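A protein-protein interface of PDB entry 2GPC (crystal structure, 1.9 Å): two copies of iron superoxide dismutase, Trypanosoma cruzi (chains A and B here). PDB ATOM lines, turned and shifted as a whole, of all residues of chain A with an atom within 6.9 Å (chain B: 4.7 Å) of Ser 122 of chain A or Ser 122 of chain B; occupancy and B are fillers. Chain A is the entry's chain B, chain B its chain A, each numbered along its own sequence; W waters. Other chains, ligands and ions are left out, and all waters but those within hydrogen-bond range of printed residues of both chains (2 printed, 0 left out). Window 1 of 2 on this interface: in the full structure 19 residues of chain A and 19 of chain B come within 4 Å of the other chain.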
ATOM      1  N   HIS A 119      16.360  10.708 -14.055  1.00  0.00           N
ATOM      2  CA  HIS A 119      16.001   9.305 -14.279  1.00  0.00           C
ATOM      3  C   HIS A 119      14.928   9.155 -15.359  1.00  0.00           C
ATOM      4  O   HIS A 119      13.837   9.699 -15.240  1.00  0.00           O
ATOM      5  CB  HIS A 119      15.523   8.608 -12.993  1.00  0.00           C
ATOM      6  CG  HIS A 119      15.448   7.121 -13.133  1.00  0.00           C
ATOM      7  ND1 HIS A 119      16.557   6.308 -13.042  1.00  0.00           N
ATOM      8  CD2 HIS A 119      14.404   6.304 -13.406  1.00  0.00           C
ATOM      9  CE1 HIS A 119      16.194   5.052 -13.232  1.00  0.00           C
ATOM     10  NE2 HIS A 119      14.892   5.025 -13.454  1.00  0.00           N
ATOM     11  N   PHE A 120      15.234   8.413 -16.412  1.00  0.00           N
ATOM     12  CA  PHE A 120      14.284   8.230 -17.499  1.00  0.00           C
ATOM     13  C   PHE A 120      13.350   7.079 -17.196  1.00  0.00           C
ATOM     14  O   PHE A 120      13.795   6.003 -16.827  1.00  0.00           O
ATOM     15  CB  PHE A 120      14.999   7.980 -18.834  1.00  0.00           C
ATOM     16  CG  PHE A 120      14.081   8.058 -20.015  1.00  0.00           C
ATOM     17  CD1 PHE A 120      13.558   9.287 -20.419  1.00  0.00           C
ATOM     18  CD2 PHE A 120      13.723   6.916 -20.716  1.00  0.00           C
ATOM     19  CE1 PHE A 120      12.698   9.373 -21.497  1.00  0.00           C
ATOM     20  CE2 PHE A 120      12.857   6.990 -21.804  1.00  0.00           C
ATOM     21  CZ  PHE A 120      12.334   8.225 -22.190  1.00  0.00           C
ATOM     22  N   GLY A 121      12.054   7.308 -17.384  1.00  0.00           N
ATOM     23  CA  GLY A 121      11.044   6.312 -17.070  1.00  0.00           C
ATOM     24  C   GLY A 121      10.766   6.240 -15.576  1.00  0.00           C
ATOM     25  O   GLY A 121      11.046   7.189 -14.822  1.00  0.00           O
ATOM     26  N   SER A 122      10.198   5.110 -15.161  1.00  0.00           N
ATOM     27  CA  SER A 122       9.804   4.880 -13.781  1.00  0.00           C
ATOM     28  C   SER A 122      11.019   4.421 -12.996  1.00  0.00           C
ATOM     29  O   SER A 122      11.815   3.651 -13.500  1.00  0.00           O
ATOM     30  CB  SER A 122       8.718   3.804 -13.722  1.00  0.00           C
ATOM     31  OG  SER A 122       7.560   4.190 -14.429  1.00  0.00           O
ATOM     32  N   GLY A 123      11.160   4.890 -11.760  1.00  0.00           N
ATOM     33  CA  GLY A 123      12.316   4.540 -10.949  1.00  0.00           C
ATOM     34  C   GLY A 123      12.381   5.200  -9.583  1.00  0.00           C
ATOM     35  O   GLY A 123      11.417   5.823  -9.113  1.00  0.00           O
ATOM     36  N   TRP A 124      13.548   5.080  -8.958  1.00  0.00           N
ATOM     37  CA  TRP A 124      13.777   5.531  -7.588  1.00  0.00           C
ATOM     38  C   TRP A 124      15.189   6.088  -7.461  1.00  0.00           C
ATOM     39  O   TRP A 124      16.140   5.497  -7.987  1.00  0.00           O
ATOM     40  CB  TRP A 124      13.647   4.353  -6.614  1.00  0.00           C
ATOM     41  CG  TRP A 124      12.317   3.652  -6.607  1.00  0.00           C
ATOM     42  CD1 TRP A 124      11.886   2.697  -7.489  1.00  0.00           C
ATOM     43  CD2 TRP A 124      11.257   3.825  -5.659  1.00  0.00           C
ATOM     44  NE1 TRP A 124      10.621   2.280  -7.153  1.00  0.00           N
ATOM     45  CE2 TRP A 124      10.208   2.960  -6.039  1.00  0.00           C
ATOM     46  CE3 TRP A 124      11.080   4.636  -4.530  1.00  0.00           C
ATOM     47  CZ2 TRP A 124       9.008   2.885  -5.340  1.00  0.00           C
ATOM     48  CZ3 TRP A 124       9.903   4.553  -3.832  1.00  0.00           C
ATOM     49  CH2 TRP A 124       8.873   3.689  -4.241  1.00  0.00           C
ATOM     50  N   THR A 141      17.528   3.126  -8.972  1.00  0.00           N
ATOM     51  CA  THR A 141      16.935   1.928  -9.532  1.00  0.00           C
ATOM     52  C   THR A 141      15.815   2.277 -10.495  1.00  0.00           C
ATOM     53  O   THR A 141      15.220   3.371 -10.446  1.00  0.00           O
ATOM     54  CB  THR A 141      16.442   0.969  -8.451  1.00  0.00           C
ATOM     55  OG1 THR A 141      15.490   1.615  -7.589  1.00  0.00           O
ATOM     56  CG2 THR A 141      17.604   0.551  -7.532  1.00  0.00           C
ATOM     57  N   HIS A 142      15.532   1.317 -11.367  1.00  0.00           N
ATOM     58  CA  HIS A 142      14.531   1.454 -12.403  1.00  0.00           C
ATOM     59  C   HIS A 142      13.361   0.548 -12.075  1.00  0.00           C
ATOM     60  O   HIS A 142      13.543  -0.535 -11.518  1.00  0.00           O
ATOM     61  CB  HIS A 142      15.150   1.054 -13.734  1.00  0.00           C
ATOM     62  CG  HIS A 142      14.397   1.546 -14.922  1.00  0.00           C
ATOM     63  ND1 HIS A 142      14.239   2.885 -15.199  1.00  0.00           N
ATOM     64  CD2 HIS A 142      13.769   0.880 -15.918  1.00  0.00           C
ATOM     65  CE1 HIS A 142      13.548   3.023 -16.316  1.00  0.00           C
ATOM     66  NE2 HIS A 142      13.253   1.822 -16.773  1.00  0.00           N
ATOM     67  N   ASP A 143      12.159   1.002 -12.404  1.00  0.00           N
ATOM     68  CA  ASP A 143      10.930   0.269 -12.115  1.00  0.00           C
ATOM     69  C   ASP A 143      10.833  -0.117 -10.628  1.00  0.00           C
ATOM     70  O   ASP A 143      10.696   0.764  -9.785  1.00  0.00           O
ATOM     71  CB  ASP A 143      10.812  -0.926 -13.056  1.00  0.00           C
ATOM     72  CG  ASP A 143      10.817  -0.515 -14.519  1.00  0.00           C
ATOM     73  OD1 ASP A 143      10.161   0.498 -14.851  1.00  0.00           O
ATOM     74  OD2 ASP A 143      11.447  -1.143 -15.399  1.00  0.00           O
ATOM     75  N   ALA A 144      10.892  -1.412 -10.304  1.00  0.00           N
ATOM     76  CA  ALA A 144      10.797  -1.883  -8.920  1.00  0.00           C
ATOM     77  C   ALA A 144      12.152  -2.227  -8.303  1.00  0.00           C
ATOM     78  O   ALA A 144      12.221  -2.695  -7.159  1.00  0.00           O
ATOM     79  CB  ALA A 144       9.856  -3.097  -8.830  1.00  0.00           C
ATOM     80  N   ASP A 160      10.738   8.440  -4.596  1.00  0.00           N
ATOM     81  CA  ASP A 160      10.007   7.767  -5.673  1.00  0.00           C
ATOM     82  C   ASP A 160       9.907   8.743  -6.838  1.00  0.00           C
ATOM     83  O   ASP A 160       9.430   9.855  -6.646  1.00  0.00           O
ATOM     84  CB  ASP A 160       8.607   7.414  -5.156  1.00  0.00           C
ATOM     85  CG  ASP A 160       7.782   6.578  -6.123  1.00  0.00           C
ATOM     86  OD1 ASP A 160       8.275   6.147  -7.197  1.00  0.00           O
ATOM     87  OD2 ASP A 160       6.581   6.300  -5.862  1.00  0.00           O
ATOM     88  N   VAL A 161      10.372   8.349  -8.022  1.00  0.00           N
ATOM     89  CA  VAL A 161      10.253   9.199  -9.217  1.00  0.00           C
ATOM     90  C   VAL A 161       9.364   8.609 -10.325  1.00  0.00           C
ATOM     91  O   VAL A 161       9.303   9.153 -11.429  1.00  0.00           O
ATOM     92  CB  VAL A 161      11.643   9.691  -9.776  1.00  0.00           C
ATOM     93  CG1 VAL A 161      12.281  10.686  -8.811  1.00  0.00           C
ATOM     94  CG2 VAL A 161      12.589   8.537 -10.080  1.00  0.00           C
ATOM     95  N   TRP A 162       8.619   7.545 -10.012  1.00  0.00           N
ATOM     96  CA  TRP A 162       7.485   7.158 -10.838  1.00  0.00           C
ATOM     97  C   TRP A 162       6.581   8.373 -10.968  1.00  0.00           C
ATOM     98  O   TRP A 162       6.436   9.159 -10.017  1.00  0.00           O
ATOM     99  CB  TRP A 162       6.674   6.024 -10.203  1.00  0.00           C
ATOM    100  CG  TRP A 162       7.254   4.671 -10.305  1.00  0.00           C
ATOM    101  CD1 TRP A 162       8.485   4.266  -9.874  1.00  0.00           C
ATOM    102  CD2 TRP A 162       6.612   3.499 -10.832  1.00  0.00           C
ATOM    103  NE1 TRP A 162       8.649   2.922 -10.110  1.00  0.00           N
ATOM    104  CE2 TRP A 162       7.513   2.423 -10.689  1.00  0.00           C
ATOM    105  CE3 TRP A 162       5.366   3.251 -11.418  1.00  0.00           C
ATOM    106  CZ2 TRP A 162       7.212   1.121 -11.121  1.00  0.00           C
ATOM    107  CZ3 TRP A 162       5.068   1.962 -11.842  1.00  0.00           C
ATOM    108  CH2 TRP A 162       5.992   0.920 -11.701  1.00  0.00           C
ATOM    109  N   GLU A 163       5.963   8.530 -12.133  1.00  0.00           N
ATOM    110  CA  GLU A 163       5.136   9.698 -12.392  1.00  0.00           C
ATOM    111  C   GLU A 163       3.923   9.821 -11.459  1.00  0.00           C
ATOM    112  O   GLU A 163       3.520  10.929 -11.121  1.00  0.00           O
ATOM    113  CB  GLU A 163       4.730   9.753 -13.872  1.00  0.00           C
ATOM    114  CG  GLU A 163       5.913  10.009 -14.794  1.00  0.00           C
ATOM    115  CD  GLU A 163       5.545  10.031 -16.265  1.00  0.00           C
ATOM    116  OE1 GLU A 163       4.738   9.186 -16.683  1.00  0.00           O
ATOM    117  OE2 GLU A 163       6.071  10.900 -16.992  1.00  0.00           O
ATOM    118  N   HIS A 164       3.366   8.701 -11.005  1.00  0.00           N
ATOM    119  CA  HIS A 164       2.229   8.747 -10.082  1.00  0.00           C
ATOM    120  C   HIS A 164       2.602   9.385  -8.726  1.00  0.00           C
ATOM    121  O   HIS A 164       1.737   9.814  -7.989  1.00  0.00           O
ATOM    122  CB  HIS A 164       1.611   7.350  -9.878  1.00  0.00           C
ATOM    123  CG  HIS A 164       2.499   6.379  -9.164  1.00  0.00           C
ATOM    124  ND1 HIS A 164       2.981   5.233  -9.757  1.00  0.00           N
ATOM    125  CD2 HIS A 164       2.975   6.373  -7.898  1.00  0.00           C
ATOM    126  CE1 HIS A 164       3.730   4.575  -8.888  1.00  0.00           C
ATOM    127  NE2 HIS A 164       3.745   5.250  -7.755  1.00  0.00           N
ATOM    128  N   ARG A 174       8.877  17.452 -12.590  1.00  0.00           N
ATOM    129  CA  ARG A 174       9.525  16.600 -11.600  1.00  0.00           C
ATOM    130  C   ARG A 174      10.558  17.378 -10.802  1.00  0.00           C
ATOM    131  O   ARG A 174      10.761  17.087  -9.627  1.00  0.00           O
ATOM    132  CB  ARG A 174      10.175  15.377 -12.245  1.00  0.00           C
ATOM    133  CG  ARG A 174      10.541  14.290 -11.226  1.00  0.00           C
ATOM    134  CD  ARG A 174      11.523  13.286 -11.729  1.00  0.00           C
ATOM    135  NE  ARG A 174      10.969  12.442 -12.784  1.00  0.00           N
ATOM    136  CZ  ARG A 174      11.669  11.536 -13.453  1.00  0.00           C
ATOM    137  NH1 ARG A 174      12.959  11.360 -13.189  1.00  0.00           N
ATOM    138  NH2 ARG A 174      11.082  10.822 -14.404  1.00  0.00           N
ATOM    139  N   HIS B 119       1.477  -3.937 -18.383  1.00  0.00           N
ATOM    140  CA  HIS B 119       2.869  -3.530 -18.581  1.00  0.00           C
ATOM    141  C   HIS B 119       3.357  -2.828 -17.322  1.00  0.00           C
ATOM    142  O   HIS B 119       2.721  -1.890 -16.850  1.00  0.00           O
ATOM    143  CB  HIS B 119       3.042  -2.607 -19.787  1.00  0.00           C
ATOM    144  CG  HIS B 119       4.470  -2.270 -20.079  1.00  0.00           C
ATOM    145  ND1 HIS B 119       5.282  -3.070 -20.858  1.00  0.00           N
ATOM    146  CD2 HIS B 119       5.242  -1.233 -19.672  1.00  0.00           C
ATOM    147  CE1 HIS B 119       6.489  -2.531 -20.927  1.00  0.00           C
ATOM    148  NE2 HIS B 119       6.490  -1.416 -20.218  1.00  0.00           N
ATOM    149  N   PHE B 120       4.464  -3.305 -16.765  1.00  0.00           N
ATOM    150  CA  PHE B 120       4.942  -2.774 -15.498  1.00  0.00           C
ATOM    151  C   PHE B 120       5.892  -1.617 -15.764  1.00  0.00           C
ATOM    152  O   PHE B 120       6.821  -1.750 -16.552  1.00  0.00           O
ATOM    153  CB  PHE B 120       5.639  -3.846 -14.678  1.00  0.00           C
ATOM    154  CG  PHE B 120       5.947  -3.403 -13.295  1.00  0.00           C
ATOM    155  CD1 PHE B 120       4.929  -3.248 -12.371  1.00  0.00           C
ATOM    156  CD2 PHE B 120       7.238  -3.075 -12.927  1.00  0.00           C
ATOM    157  CE1 PHE B 120       5.201  -2.812 -11.085  1.00  0.00           C
ATOM    158  CE2 PHE B 120       7.516  -2.638 -11.634  1.00  0.00           C
ATOM    159  CZ  PHE B 120       6.497  -2.499 -10.723  1.00  0.00           C
ATOM    160  N   GLY B 121       5.642  -0.485 -15.119  1.00  0.00           N
ATOM    161  CA  GLY B 121       6.409   0.728 -15.358  1.00  0.00           C
ATOM    162  C   GLY B 121       5.948   1.447 -16.616  1.00  0.00           C
ATOM    163  O   GLY B 121       4.830   1.245 -17.079  1.00  0.00           O
ATOM    164  N   SER B 122       6.828   2.288 -17.144  1.00  0.00           N
ATOM    165  CA  SER B 122       6.560   3.137 -18.301  1.00  0.00           C
ATOM    166  C   SER B 122       6.731   2.340 -19.576  1.00  0.00           C
ATOM    167  O   SER B 122       7.699   1.581 -19.714  1.00  0.00           O
ATOM    168  CB  SER B 122       7.543   4.308 -18.317  1.00  0.00           C
ATOM    169  OG  SER B 122       7.402   5.138 -17.173  1.00  0.00           O
ATOM    170  N   GLY B 123       5.810   2.512 -20.516  1.00  0.00           N
ATOM    171  CA  GLY B 123       5.895   1.780 -21.764  1.00  0.00           C
ATOM    172  C   GLY B 123       4.810   2.063 -22.780  1.00  0.00           C
ATOM    173  O   GLY B 123       4.088   3.040 -22.680  1.00  0.00           O
ATOM    174  N   THR B 141       6.772  -2.298 -25.787  1.00  0.00           N
ATOM    175  CA  THR B 141       8.104  -1.759 -25.558  1.00  0.00           C
ATOM    176  C   THR B 141       8.146  -1.083 -24.202  1.00  0.00           C
ATOM    177  O   THR B 141       7.117  -0.656 -23.669  1.00  0.00           O
ATOM    178  CB  THR B 141       8.543  -0.814 -26.691  1.00  0.00           C
ATOM    179  OG1 THR B 141       7.643   0.302 -26.812  1.00  0.00           O
ATOM    180  CG2 THR B 141       8.485  -1.518 -28.032  1.00  0.00           C
ATOM    181  N   HIS B 142       9.342  -1.029 -23.633  1.00  0.00           N
ATOM    182  CA  HIS B 142       9.540  -0.465 -22.319  1.00  0.00           C
ATOM    183  C   HIS B 142      10.221   0.887 -22.487  1.00  0.00           C
ATOM    184  O   HIS B 142      11.091   1.053 -23.345  1.00  0.00           O
ATOM    185  CB  HIS B 142      10.404  -1.413 -21.481  1.00  0.00           C
ATOM    186  CG  HIS B 142      10.369  -1.134 -20.014  1.00  0.00           C
ATOM    187  ND1 HIS B 142       9.195  -1.106 -19.290  1.00  0.00           N
ATOM    188  CD2 HIS B 142      11.366  -0.884 -19.128  1.00  0.00           C
ATOM    189  CE1 HIS B 142       9.472  -0.856 -18.022  1.00  0.00           C
ATOM    190  NE2 HIS B 142      10.781  -0.725 -17.897  1.00  0.00           N
ATOM    191  N   ASP B 143       9.810   1.838 -21.660  1.00  0.00           N
ATOM    192  CA  ASP B 143      10.345   3.198 -21.670  1.00  0.00           C
ATOM    193  C   ASP B 143      10.157   3.854 -23.037  1.00  0.00           C
ATOM    194  O   ASP B 143       9.016   4.112 -23.420  1.00  0.00           O
ATOM    195  CB  ASP B 143      11.788   3.203 -21.178  1.00  0.00           C
ATOM    196  CG  ASP B 143      11.909   2.670 -19.773  1.00  0.00           C
ATOM    197  OD1 ASP B 143      11.011   2.954 -18.946  1.00  0.00           O
ATOM    198  OD2 ASP B 143      12.858   1.965 -19.396  1.00  0.00           O
ATOM    199  N   TRP B 162       2.679   5.057 -20.364  1.00  0.00           N
ATOM    200  CA  TRP B 162       3.325   5.917 -19.378  1.00  0.00           C
ATOM    201  C   TRP B 162       2.203   6.538 -18.564  1.00  0.00           C
ATOM    202  O   TRP B 162       1.161   6.904 -19.120  1.00  0.00           O
ATOM    203  CB  TRP B 162       4.158   7.028 -20.041  1.00  0.00           C
ATOM    204  CG  TRP B 162       5.498   6.612 -20.601  1.00  0.00           C
ATOM    205  CD1 TRP B 162       5.732   5.695 -21.579  1.00  0.00           C
ATOM    206  CD2 TRP B 162       6.780   7.146 -20.244  1.00  0.00           C
ATOM    207  NE1 TRP B 162       7.076   5.613 -21.854  1.00  0.00           N
ATOM    208  CE2 TRP B 162       7.748   6.493 -21.046  1.00  0.00           C
ATOM    209  CE3 TRP B 162       7.213   8.116 -19.329  1.00  0.00           C
ATOM    210  CZ2 TRP B 162       9.114   6.765 -20.949  1.00  0.00           C
ATOM    211  CZ3 TRP B 162       8.560   8.383 -19.231  1.00  0.00           C
ATOM    212  CH2 TRP B 162       9.503   7.707 -20.036  1.00  0.00           C
HETATM  213  O   HOH W   1       9.716   2.495 -16.595  1.00  0.00           O
HETATM  214  O   HOH W   2       5.276   6.473 -16.458  1.00  0.00           O
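NE2 of His 119 of chain A sits at hydrogen-bond distance from O of Ser 122 of chain A. The indole nitrogen (NE1) of Trp 124 of chain A is in hydrogen-bond range of the backbone carbonyl oxygen (O) of Asp 143 of chain A (3.0 Å). ND1 of His 142 of chain B sits at hydrogen-bond distance from NE2 of His 119 of chain B (2.9 Å). O of Ser 122 of chain B is in hydrogen-bond range of NE2 of His 119 of chain B (3.3 Å). OD1 of Asp 160 of chain A is in hydrogen-bond range of N of Trp 162 of chain A (3.2 Å). O of Gly 123 of chain B lies close to N of Trp 162 of chain B, at 3.4 Å.
Ser 122 of chain A touches two residues of chain B. Ser 122 of chain B touches two residues of chain A. Of the printed residues of chain A, Gly 121 of chain B touches Ser 122, Asp 143 and Trp 162. Of the printed residues of chain B, Trp 162 of chain A touches Phe 120 (3.6 Å) and Gly 121 (3.7 Å). Printed residues of chain A within 4 Å of Trp 162 of chain B: Phe 120, Gly 121 and Glu 163. Thr 141 of chain B touches none of the printed residues of chain A. His 119 of chain A touches none of the printed residues of chain B. The nearest residue of chain B that does not touch Ser 122 of chain A is Asp 143 of chain B (4.4 Å). The nearest printed residue of chain A that does not touch His 142 of chain B is Ser 122 of chain A (6.3 Å).
The side-chain carboxylate (OD2) of Asp 143 of chain B sits at hydrogen-bond distance from a ring nitrogen (NE2) of His 142 of chain A, at 2.7 Å. The side-chain hydroxyl of Ser 122 of chain A sits at hydrogen-bond distance from the side-chain hydroxyl of Ser 122 of chain B (2.9 Å). NE2 of His 142 of chain B sits at hydrogen-bond distance from OD2 of Asp 143 of chain A (2.6 Å).
Gly 121 of chain A touches Ser 122 of chain B. OD1 of Asp 143 of chain B touches CA of Gly 121 of chain A, 3.8 Å away. Gly 121 of chain A touches Trp 162 of chain B (CA to CH2, 3.6 Å). OG of Ser 122 of chain A touches CA of Gly 121 of chain B, 3.8 Å away. His 142 of chain B touches His 142 of chain A (NE2 to NE2, 3.7 Å). CB of Asp 143 of chain A touches CE2 of Phe 120 of chain B (3.98 Å). Asp 143 of chain A touches Gly 121 of chain B (OD1 to CA, 3.8 Å). Ala 144 of chain A touches Phe 120 of chain B. Trp 162 of chain A touches Phe 120 of chain B. Trp 162 of chain A touches Gly 121 of chain B (CH2 to CA, 3.7 Å).
Water W2 bridges OG of Ser 122 of chain B and OE1 of Glu 163 of chain A. Water W1 lies within hydrogen-bond range of the side-chain carboxylate of Asp 143 of chain A (2.7 Å), the side-chain carboxylate of Asp 143 of chain B (2.7 Å), the backbone NH of Ser 122 of chain B (2.9 Å) and the backbone NH of Ser 122 of chain A (3.0 Å).
Phe 120 of chain A touches Asp 143 of chain B, and with the chains exchanged Asp 143 of chain A touches Phe 120 of chain B. Gly 121 of chain A touches Ser 122 of chain B, and with the chains exchanged Ser 122 of chain A touches Gly 121 of chain B. Gly 121 of chain A touches Asp 143 of chain B, and with the chains exchanged Asp 143 of chain A touches Gly 121 of chain B. His 142 of chain A touches Asp 143 of chain B, and with the chains exchanged Asp 143 of chain A touches His 142 of chain B. 9 positions are printed for both chains. Of the 16 pairs that touch across the chains among the printed residues, 14 have their exchanged pair printed and touching as well.
Of the 16 printed residues of chain A, 8 touch a printed residue of chain B. Hydrophobic or aromatic side chains of chain A that line the printed part of chain B: Phe 120, His 142, Ala 144 and Trp 162. Hydrophobic or aromatic side chains of chain B that line the printed part of chain A: Phe 120, His 142 and Trp 162. Among the printed residues, 16 pairs touch across the chains.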
